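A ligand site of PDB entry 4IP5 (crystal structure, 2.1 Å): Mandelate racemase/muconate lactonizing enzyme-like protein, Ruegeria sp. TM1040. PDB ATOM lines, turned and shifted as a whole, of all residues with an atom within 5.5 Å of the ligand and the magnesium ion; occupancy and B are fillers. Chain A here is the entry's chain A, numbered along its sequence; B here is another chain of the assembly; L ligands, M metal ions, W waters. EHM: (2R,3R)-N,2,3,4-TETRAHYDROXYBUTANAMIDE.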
ATOM      1  N   GLY A  22     -11.203 -25.480  18.075  1.00  0.00           N
ATOM      2  CA  GLY A  22     -12.507 -24.969  17.685  1.00  0.00           C
ATOM      3  C   GLY A  22     -13.639 -25.351  18.624  1.00  0.00           C
ATOM      4  O   GLY A  22     -14.744 -24.815  18.516  1.00  0.00           O
ATOM      5  N   SER A  23     -13.365 -26.281  19.542  1.00  0.00           N
ATOM      6  CA  SER A  23     -14.430 -26.815  20.409  1.00  0.00           C
ATOM      7  C   SER A  23     -15.050 -25.761  21.333  1.00  0.00           C
ATOM      8  O   SER A  23     -14.337 -24.910  21.865  1.00  0.00           O
ATOM      9  CB  SER A  23     -13.896 -27.982  21.250  1.00  0.00           C
ATOM     10  OG  SER A  23     -12.761 -27.582  22.009  1.00  0.00           O
ATOM     11  N   ASP A  24     -16.359 -25.829  21.511  1.00  0.00           N
ATOM     12  CA  ASP A  24     -17.054 -24.889  22.391  1.00  0.00           C
ATOM     13  C   ASP A  24     -18.271 -25.541  23.057  1.00  0.00           C
ATOM     14  O   ASP A  24     -18.502 -26.740  22.905  1.00  0.00           O
ATOM     15  CB  ASP A  24     -17.467 -23.644  21.602  1.00  0.00           C
ATOM     16  CG  ASP A  24     -18.389 -23.977  20.444  1.00  0.00           C
ATOM     17  OD1 ASP A  24     -19.504 -24.491  20.701  1.00  0.00           O
ATOM     18  OD2 ASP A  24     -18.007 -23.714  19.279  1.00  0.00           O
ATOM     19  N   ASN A  27     -20.633 -26.617  20.099  1.00  0.00           N
ATOM     20  CA  ASN A  27     -19.990 -27.453  19.095  1.00  0.00           C
ATOM     21  C   ASN A  27     -18.791 -28.155  19.711  1.00  0.00           C
ATOM     22  O   ASN A  27     -17.682 -27.609  19.743  1.00  0.00           O
ATOM     23  CB  ASN A  27     -19.543 -26.576  17.907  1.00  0.00           C
ATOM     24  CG  ASN A  27     -20.625 -25.580  17.477  1.00  0.00           C
ATOM     25  OD1 ASN A  27     -21.685 -25.994  17.008  1.00  0.00           O
ATOM     26  ND2 ASN A  27     -20.363 -24.293  17.654  1.00  0.00           N
ATOM     27  N   PRO A  30     -16.029 -29.753  16.322  1.00  0.00           N
ATOM     28  CA  PRO A  30     -16.160 -29.278  14.946  1.00  0.00           C
ATOM     29  C   PRO A  30     -15.012 -29.751  14.054  1.00  0.00           C
ATOM     30  O   PRO A  30     -13.853 -29.793  14.490  1.00  0.00           O
ATOM     31  CB  PRO A  30     -16.116 -27.756  15.101  1.00  0.00           C
ATOM     32  CG  PRO A  30     -15.332 -27.533  16.363  1.00  0.00           C
ATOM     33  CD  PRO A  30     -15.744 -28.656  17.270  1.00  0.00           C
ATOM     34  N   TYR A  32     -13.496 -28.285  10.978  1.00  0.00           N
ATOM     35  CA  TYR A  32     -13.422 -27.082  10.161  1.00  0.00           C
ATOM     36  C   TYR A  32     -13.459 -27.393   8.673  1.00  0.00           C
ATOM     37  O   TYR A  32     -12.609 -28.132   8.160  1.00  0.00           O
ATOM     38  CB  TYR A  32     -12.191 -26.251  10.536  1.00  0.00           C
ATOM     39  CG  TYR A  32     -12.380 -25.415  11.779  1.00  0.00           C
ATOM     40  CD1 TYR A  32     -13.438 -25.657  12.662  1.00  0.00           C
ATOM     41  CD2 TYR A  32     -11.512 -24.361  12.076  1.00  0.00           C
ATOM     42  CE1 TYR A  32     -13.619 -24.875  13.801  1.00  0.00           C
ATOM     43  CE2 TYR A  32     -11.679 -23.589  13.215  1.00  0.00           C
ATOM     44  CZ  TYR A  32     -12.735 -23.839  14.063  1.00  0.00           C
ATOM     45  OH  TYR A  32     -12.918 -23.051  15.180  1.00  0.00           O
ATOM     46  N   PHE A  52     -17.639 -21.015   5.286  1.00  0.00           N
ATOM     47  CA  PHE A  52     -17.121 -21.876   6.356  1.00  0.00           C
ATOM     48  C   PHE A  52     -18.209 -22.666   7.076  1.00  0.00           C
ATOM     49  O   PHE A  52     -19.235 -22.089   7.469  1.00  0.00           O
ATOM     50  CB  PHE A  52     -16.337 -21.019   7.361  1.00  0.00           C
ATOM     51  CG  PHE A  52     -16.034 -21.726   8.667  1.00  0.00           C
ATOM     52  CD1 PHE A  52     -15.094 -22.760   8.703  1.00  0.00           C
ATOM     53  CD2 PHE A  52     -16.669 -21.350   9.844  1.00  0.00           C
ATOM     54  CE1 PHE A  52     -14.820 -23.422   9.894  1.00  0.00           C
ATOM     55  CE2 PHE A  52     -16.388 -22.003  11.043  1.00  0.00           C
ATOM     56  CZ  PHE A  52     -15.458 -23.040  11.064  1.00  0.00           C
ATOM     57  N   ILE A  54     -18.641 -26.518   9.813  1.00  0.00           N
ATOM     58  CA  ILE A  54     -17.888 -27.355  10.755  1.00  0.00           C
ATOM     59  C   ILE A  54     -18.070 -28.856  10.529  1.00  0.00           C
ATOM     60  O   ILE A  54     -18.023 -29.637  11.478  1.00  0.00           O
ATOM     61  CB  ILE A  54     -18.175 -26.980  12.220  1.00  0.00           C
ATOM     62  CG1 ILE A  54     -19.684 -27.052  12.519  1.00  0.00           C
ATOM     63  CG2 ILE A  54     -17.647 -25.571  12.533  1.00  0.00           C
ATOM     64  CD1 ILE A  54     -20.031 -26.941  14.009  1.00  0.00           C
ATOM     65  N   TYR A 186      -7.456  -9.633  18.539  1.00  0.00           N
ATOM     66  CA  TYR A 186      -7.440 -10.462  19.731  1.00  0.00           C
ATOM     67  C   TYR A 186      -7.270 -11.910  19.346  1.00  0.00           C
ATOM     68  O   TYR A 186      -7.416 -12.258  18.178  1.00  0.00           O
ATOM     69  CB  TYR A 186      -8.704 -10.277  20.578  1.00  0.00           C
ATOM     70  CG  TYR A 186      -9.981 -10.912  20.033  1.00  0.00           C
ATOM     71  CD1 TYR A 186     -10.292 -12.247  20.311  1.00  0.00           C
ATOM     72  CD2 TYR A 186     -10.901 -10.161  19.308  1.00  0.00           C
ATOM     73  CE1 TYR A 186     -11.473 -12.820  19.856  1.00  0.00           C
ATOM     74  CE2 TYR A 186     -12.097 -10.724  18.853  1.00  0.00           C
ATOM     75  CZ  TYR A 186     -12.373 -12.039  19.122  1.00  0.00           C
ATOM     76  OH  TYR A 186     -13.550 -12.595  18.652  1.00  0.00           O
ATOM     77  N   THR A 188      -8.194 -16.113  20.060  1.00  0.00           N
ATOM     78  CA  THR A 188      -9.055 -17.140  20.633  1.00  0.00           C
ATOM     79  C   THR A 188      -8.276 -18.452  20.729  1.00  0.00           C
ATOM     80  O   THR A 188      -8.791 -19.497  21.152  1.00  0.00           O
ATOM     81  CB  THR A 188     -10.314 -17.334  19.753  1.00  0.00           C
ATOM     82  OG1 THR A 188     -10.853 -16.045  19.416  1.00  0.00           O
ATOM     83  CG2 THR A 188     -11.399 -18.160  20.482  1.00  0.00           C
ATOM     84  N   TRP A 192     -10.307 -22.603  23.461  1.00  0.00           N
ATOM     85  CA  TRP A 192     -11.208 -23.709  23.117  1.00  0.00           C
ATOM     86  C   TRP A 192     -11.568 -24.590  24.312  1.00  0.00           C
ATOM     87  O   TRP A 192     -10.712 -24.915  25.142  1.00  0.00           O
ATOM     88  CB  TRP A 192     -10.665 -24.544  21.943  1.00  0.00           C
ATOM     89  CG  TRP A 192     -10.289 -23.679  20.756  1.00  0.00           C
ATOM     90  CD1 TRP A 192      -9.043 -23.518  20.229  1.00  0.00           C
ATOM     91  CD2 TRP A 192     -11.163 -22.852  19.971  1.00  0.00           C
ATOM     92  NE1 TRP A 192      -9.085 -22.641  19.170  1.00  0.00           N
ATOM     93  CE2 TRP A 192     -10.384 -22.219  18.989  1.00  0.00           C
ATOM     94  CE3 TRP A 192     -12.539 -22.580  20.015  1.00  0.00           C
ATOM     95  CZ2 TRP A 192     -10.925 -21.347  18.045  1.00  0.00           C
ATOM     96  CZ3 TRP A 192     -13.076 -21.721  19.072  1.00  0.00           C
ATOM     97  CH2 TRP A 192     -12.275 -21.117  18.098  1.00  0.00           C
ATOM     98  N   LYS A 216      -9.752 -14.435  24.248  1.00  0.00           N
ATOM     99  CA  LYS A 216     -11.128 -14.918  24.378  1.00  0.00           C
ATOM    100  C   LYS A 216     -11.183 -16.385  24.794  1.00  0.00           C
ATOM    101  O   LYS A 216     -10.390 -17.197  24.333  1.00  0.00           O
ATOM    102  CB  LYS A 216     -11.925 -14.685  23.091  1.00  0.00           C
ATOM    103  CG  LYS A 216     -13.436 -14.953  23.234  1.00  0.00           C
ATOM    104  CD  LYS A 216     -14.226 -14.511  22.003  1.00  0.00           C
ATOM    105  CE  LYS A 216     -13.948 -15.411  20.798  1.00  0.00           C
ATOM    106  NZ  LYS A 216     -14.733 -14.981  19.596  1.00  0.00           N
ATOM    107  N   LYS A 218     -13.775 -19.905  25.764  1.00  0.00           N
ATOM    108  CA  LYS A 218     -15.075 -20.540  25.680  1.00  0.00           C
ATOM    109  C   LYS A 218     -15.632 -20.838  27.080  1.00  0.00           C
ATOM    110  O   LYS A 218     -14.875 -21.182  27.996  1.00  0.00           O
ATOM    111  CB  LYS A 218     -14.987 -21.823  24.864  1.00  0.00           C
ATOM    112  CG  LYS A 218     -14.624 -21.609  23.404  1.00  0.00           C
ATOM    113  CD  LYS A 218     -15.596 -20.632  22.756  1.00  0.00           C
ATOM    114  CE  LYS A 218     -15.294 -20.457  21.283  1.00  0.00           C
ATOM    115  NZ  LYS A 218     -16.311 -19.644  20.563  1.00  0.00           N
ATOM    116  N   ASP A 246     -17.222 -16.512  25.487  1.00  0.00           N
ATOM    117  CA  ASP A 246     -18.122 -16.872  24.392  1.00  0.00           C
ATOM    118  C   ASP A 246     -18.879 -18.123  24.789  1.00  0.00           C
ATOM    119  O   ASP A 246     -18.248 -19.152  25.059  1.00  0.00           O
ATOM    120  CB  ASP A 246     -17.286 -17.159  23.141  1.00  0.00           C
ATOM    121  CG  ASP A 246     -18.137 -17.317  21.876  1.00  0.00           C
ATOM    122  OD1 ASP A 246     -19.387 -17.458  21.957  1.00  0.00           O
ATOM    123  OD2 ASP A 246     -17.529 -17.306  20.784  1.00  0.00           O
ATOM    124  N   ASN A 248     -21.449 -19.424  22.803  1.00  0.00           N
ATOM    125  CA  ASN A 248     -21.936 -20.086  21.591  1.00  0.00           C
ATOM    126  C   ASN A 248     -23.424 -20.448  21.603  1.00  0.00           C
ATOM    127  O   ASN A 248     -23.808 -21.541  21.186  1.00  0.00           O
ATOM    128  CB  ASN A 248     -21.047 -21.311  21.273  1.00  0.00           C
ATOM    129  CG  ASN A 248     -19.692 -20.905  20.715  1.00  0.00           C
ATOM    130  OD1 ASN A 248     -18.731 -20.723  21.469  1.00  0.00           O
ATOM    131  ND2 ASN A 248     -19.627 -20.716  19.406  1.00  0.00           N
ATOM    132  N   GLU A 272     -20.040 -13.259  24.540  1.00  0.00           N
ATOM    133  CA  GLU A 272     -20.369 -13.390  23.116  1.00  0.00           C
ATOM    134  C   GLU A 272     -21.433 -14.455  22.920  1.00  0.00           C
ATOM    135  O   GLU A 272     -21.376 -15.531  23.540  1.00  0.00           O
ATOM    136  CB  GLU A 272     -19.105 -13.740  22.318  1.00  0.00           C
ATOM    137  CG  GLU A 272     -19.384 -14.171  20.878  1.00  0.00           C
ATOM    138  CD  GLU A 272     -18.114 -14.285  20.049  1.00  0.00           C
ATOM    139  OE1 GLU A 272     -17.087 -13.675  20.440  1.00  0.00           O
ATOM    140  OE2 GLU A 272     -18.147 -14.979  19.007  1.00  0.00           O
ATOM    141  N   GLU A 273     -22.404 -14.167  22.056  1.00  0.00           N
ATOM    142  CA  GLU A 273     -23.524 -15.087  21.812  1.00  0.00           C
ATOM    143  C   GLU A 273     -24.075 -15.743  23.091  1.00  0.00           C
ATOM    144  O   GLU A 273     -24.021 -16.974  23.251  1.00  0.00           O
ATOM    145  CB  GLU A 273     -23.097 -16.172  20.832  1.00  0.00           C
ATOM    146  CG  GLU A 273     -22.762 -15.655  19.439  1.00  0.00           C
ATOM    147  CD  GLU A 273     -23.036 -16.729  18.398  1.00  0.00           C
ATOM    148  OE1 GLU A 273     -22.203 -17.657  18.274  1.00  0.00           O
ATOM    149  OE2 GLU A 273     -24.080 -16.660  17.713  1.00  0.00           O
ATOM    150  N   GLU A 299     -21.651 -13.688  14.599  1.00  0.00           N
ATOM    151  CA  GLU A 299     -20.986 -14.633  13.698  1.00  0.00           C
ATOM    152  C   GLU A 299     -21.985 -15.504  12.935  1.00  0.00           C
ATOM    153  O   GLU A 299     -21.711 -15.910  11.802  1.00  0.00           O
ATOM    154  CB  GLU A 299     -19.967 -15.505  14.434  1.00  0.00           C
ATOM    155  CG  GLU A 299     -20.565 -16.619  15.278  1.00  0.00           C
ATOM    156  CD  GLU A 299     -19.490 -17.386  16.032  1.00  0.00           C
ATOM    157  OE1 GLU A 299     -18.798 -16.773  16.884  1.00  0.00           O
ATOM    158  OE2 GLU A 299     -19.316 -18.586  15.765  1.00  0.00           O
ATOM    159  N   HIS A 349     -15.802 -11.702  13.518  1.00  0.00           N
ATOM    160  CA  HIS A 349     -15.567 -13.092  13.832  1.00  0.00           C
ATOM    161  C   HIS A 349     -14.575 -13.637  12.808  1.00  0.00           C
ATOM    162  O   HIS A 349     -14.627 -13.276  11.634  1.00  0.00           O
ATOM    163  CB  HIS A 349     -16.881 -13.862  13.731  1.00  0.00           C
ATOM    164  CG  HIS A 349     -16.720 -15.352  13.751  1.00  0.00           C
ATOM    165  ND1 HIS A 349     -16.904 -16.130  12.621  1.00  0.00           N
ATOM    166  CD2 HIS A 349     -16.440 -16.208  14.759  1.00  0.00           C
ATOM    167  CE1 HIS A 349     -16.724 -17.405  12.944  1.00  0.00           C
ATOM    168  NE2 HIS A 349     -16.438 -17.476  14.233  1.00  0.00           N
ATOM    169  N   ALA A 350     -13.687 -14.516  13.270  1.00  0.00           N
ATOM    170  CA  ALA A 350     -12.673 -15.085  12.382  1.00  0.00           C
ATOM    171  C   ALA A 350     -12.344 -16.521  12.760  1.00  0.00           C
ATOM    172  O   ALA A 350     -13.178 -17.227  13.342  1.00  0.00           O
ATOM    173  CB  ALA A 350     -11.408 -14.217  12.380  1.00  0.00           C
ATOM    174  N   GLU A 380     -10.961 -10.583  15.404  1.00  0.00           N
ATOM    175  CA  GLU A 380     -10.609 -11.874  15.968  1.00  0.00           C
ATOM    176  C   GLU A 380      -9.439 -12.456  15.179  1.00  0.00           C
ATOM    177  O   GLU A 380      -9.313 -12.225  13.967  1.00  0.00           O
ATOM    178  CB  GLU A 380     -11.793 -12.842  15.938  1.00  0.00           C
ATOM    179  CG  GLU A 380     -11.482 -14.192  16.575  1.00  0.00           C
ATOM    180  CD  GLU A 380     -12.699 -15.089  16.755  1.00  0.00           C
ATOM    181  OE1 GLU A 380     -13.755 -14.849  16.099  1.00  0.00           O
ATOM    182  OE2 GLU A 380     -12.611 -16.040  17.569  1.00  0.00           O
ATOM    183  N   TRP B  99     -25.056 -25.577  12.165  1.00  0.00           N
ATOM    184  CA  TRP B  99     -24.229 -24.518  11.591  1.00  0.00           C
ATOM    185  C   TRP B  99     -24.808 -24.014  10.272  1.00  0.00           C
ATOM    186  O   TRP B  99     -24.652 -22.839   9.909  1.00  0.00           O
ATOM    187  CB  TRP B  99     -22.810 -25.023  11.357  1.00  0.00           C
ATOM    188  CG  TRP B  99     -21.871 -23.901  11.128  1.00  0.00           C
ATOM    189  CD1 TRP B  99     -21.621 -23.265   9.949  1.00  0.00           C
ATOM    190  CD2 TRP B  99     -21.085 -23.247  12.133  1.00  0.00           C
ATOM    191  NE1 TRP B  99     -20.699 -22.247  10.155  1.00  0.00           N
ATOM    192  CE2 TRP B  99     -20.354 -22.219  11.483  1.00  0.00           C
ATOM    193  CE3 TRP B  99     -20.897 -23.451  13.506  1.00  0.00           C
ATOM    194  CZ2 TRP B  99     -19.470 -21.388  12.170  1.00  0.00           C
ATOM    195  CZ3 TRP B  99     -20.016 -22.613  14.186  1.00  0.00           C
ATOM    196  CH2 TRP B  99     -19.320 -21.607  13.515  1.00  0.00           C
HETATM  197  O4  EHM L   1     -15.281 -23.277  16.464  1.00  0.00           O
HETATM  198  C4  EHM L   1     -16.549 -22.736  16.307  1.00  0.00           C
HETATM  199  C3  EHM L   1     -16.883 -21.538  17.162  1.00  0.00           C
HETATM  200  O3  EHM L   1     -16.405 -21.748  18.442  1.00  0.00           O
HETATM  201  C2  EHM L   1     -16.330 -20.234  16.594  1.00  0.00           C
HETATM  202  O2  EHM L   1     -16.940 -20.012  15.357  1.00  0.00           O
HETATM  203  C1  EHM L   1     -16.623 -19.057  17.485  1.00  0.00           C
HETATM  204  O1  EHM L   1     -17.630 -19.022  18.181  1.00  0.00           O
HETATM  205  N   EHM L   1     -15.721 -17.940  17.510  1.00  0.00           N
HETATM  206  ON  EHM L   1     -15.999 -16.920  18.273  1.00  0.00           O
HETATM  207 MG    MG M   1     -17.946 -17.038  18.780  1.00  0.00          MG
HETATM  208  O   HOH W   1     -19.868 -17.501  19.335  1.00  0.00           O
HETATM  209  O   HOH W   2     -16.251 -13.813  17.017  1.00  0.00           O
HETATM  210  O   HOH W   3     -13.398 -18.190  15.841  1.00  0.00           O
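Lys 216 touches the magnesium ion (NZ to MG, 3.9 Å).
Lys 218 touches the magnesium ion (NZ to MG, 3.6 Å).
Five residues have an atom within 4 Å of the magnesium ion: Lys 216, Lys 218, Asp 246, Glu 272 and Glu 299.
Along chain A the residues within 4 Å of the magnesium ion span positions 216 to 299.
The magnesium ion is bound by ON of the ligand, 2.0 Å away.
Water W1 binds the magnesium ion, at 2.1 Å.
The side-chain carboxylate (OD2) of Asp 246 is bound to the magnesium ion (2.1 Å).
OE2 of Glu 272 is bound to the magnesium ion (2.1 Å).
The side-chain carboxylate (OE1) of Glu 299 binds the magnesium ion (2.1 Å).
The magnesium ion is bound by O1 of the ligand.
The magnesium ion has six donor atoms within binding distance.
Water W1 lies within hydrogen-bond range of OE1 of Glu 273 (2.6 Å), OD1 of Asp 246 (2.7 Å) and ND2 of Asn 248 (3.2 Å).
Water W3 lies within hydrogen-bond range of O of Ala 350, OE2 of Glu 380 and N of the ligand.
Water W2 lies within hydrogen-bond range of OE1 of Glu 380, NZ of Lys 216 and OH of Tyr 186.
The side-chain carboxylate (OD2) of Asp 246 sits close to the side-chain amino group (NZ) of Lys 218 (2.6 Å).
OE1 of Glu 272 lies within salt-bridge range of NZ of Lys 216 (2.8 Å).
The side-chain hydroxyl of Tyr 186 is in hydrogen-bond range of the side-chain amino group of Lys 216 (2.8 Å).
The side-chain carboxylate (OD2) of Asp 24 sits at hydrogen-bond distance from the side-chain amide nitrogen (ND2) of Asn 248, 3.4 Å away.
NE1 of Trp 99 of chain B lies within hydrogen-bond range of O of Phe 52, 3.1 Å away.
OE1 of Glu 380 is in hydrogen-bond range of N of Ala 350 (2.8 Å).
OH of Tyr 186 sits close to OE1 of Glu 380, at 3.4 Å.
OG1 of Thr 188 lies within hydrogen-bond range of OE2 of Glu 380.
An oxygen (O4) of the ligand is in hydrogen-bond range of the backbone carbonyl oxygen of Gly 22 (2.6 Å).
ON of the ligand sits close to NZ of Lys 216, 2.7 Å away.
The side-chain carboxylate of Asp 24 is in hydrogen-bond range of an oxygen (O3) of the ligand (2.7 Å).
OH of Tyr 32 is in hydrogen-bond range of O4 of the ligand, 2.7 Å away.
O3 of the ligand is in hydrogen-bond range of NZ of Lys 218, at 3.0 Å.
NE2 of His 349 sits at hydrogen-bond distance from O2 of the ligand, 2.8 Å away.
The side-chain amide nitrogen (ND2) of Asn 248 lies close to an oxygen (O1) of the ligand.
Trp 192 touches the ligand.
Glu 380 touches the ligand (OE2 to ON, 3.6 Å).
Trp 99 of chain B touches the ligand (CH2 to O2, 3.4 Å).
Of the 22 residues printed, 13 come within 4 Å of the ligand.
Along chain A the residues within 4 Å of the ligand span positions 22 to 380.
The nearest printed residue that does not touch the ligand is Pro 30 (4.3 Å).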
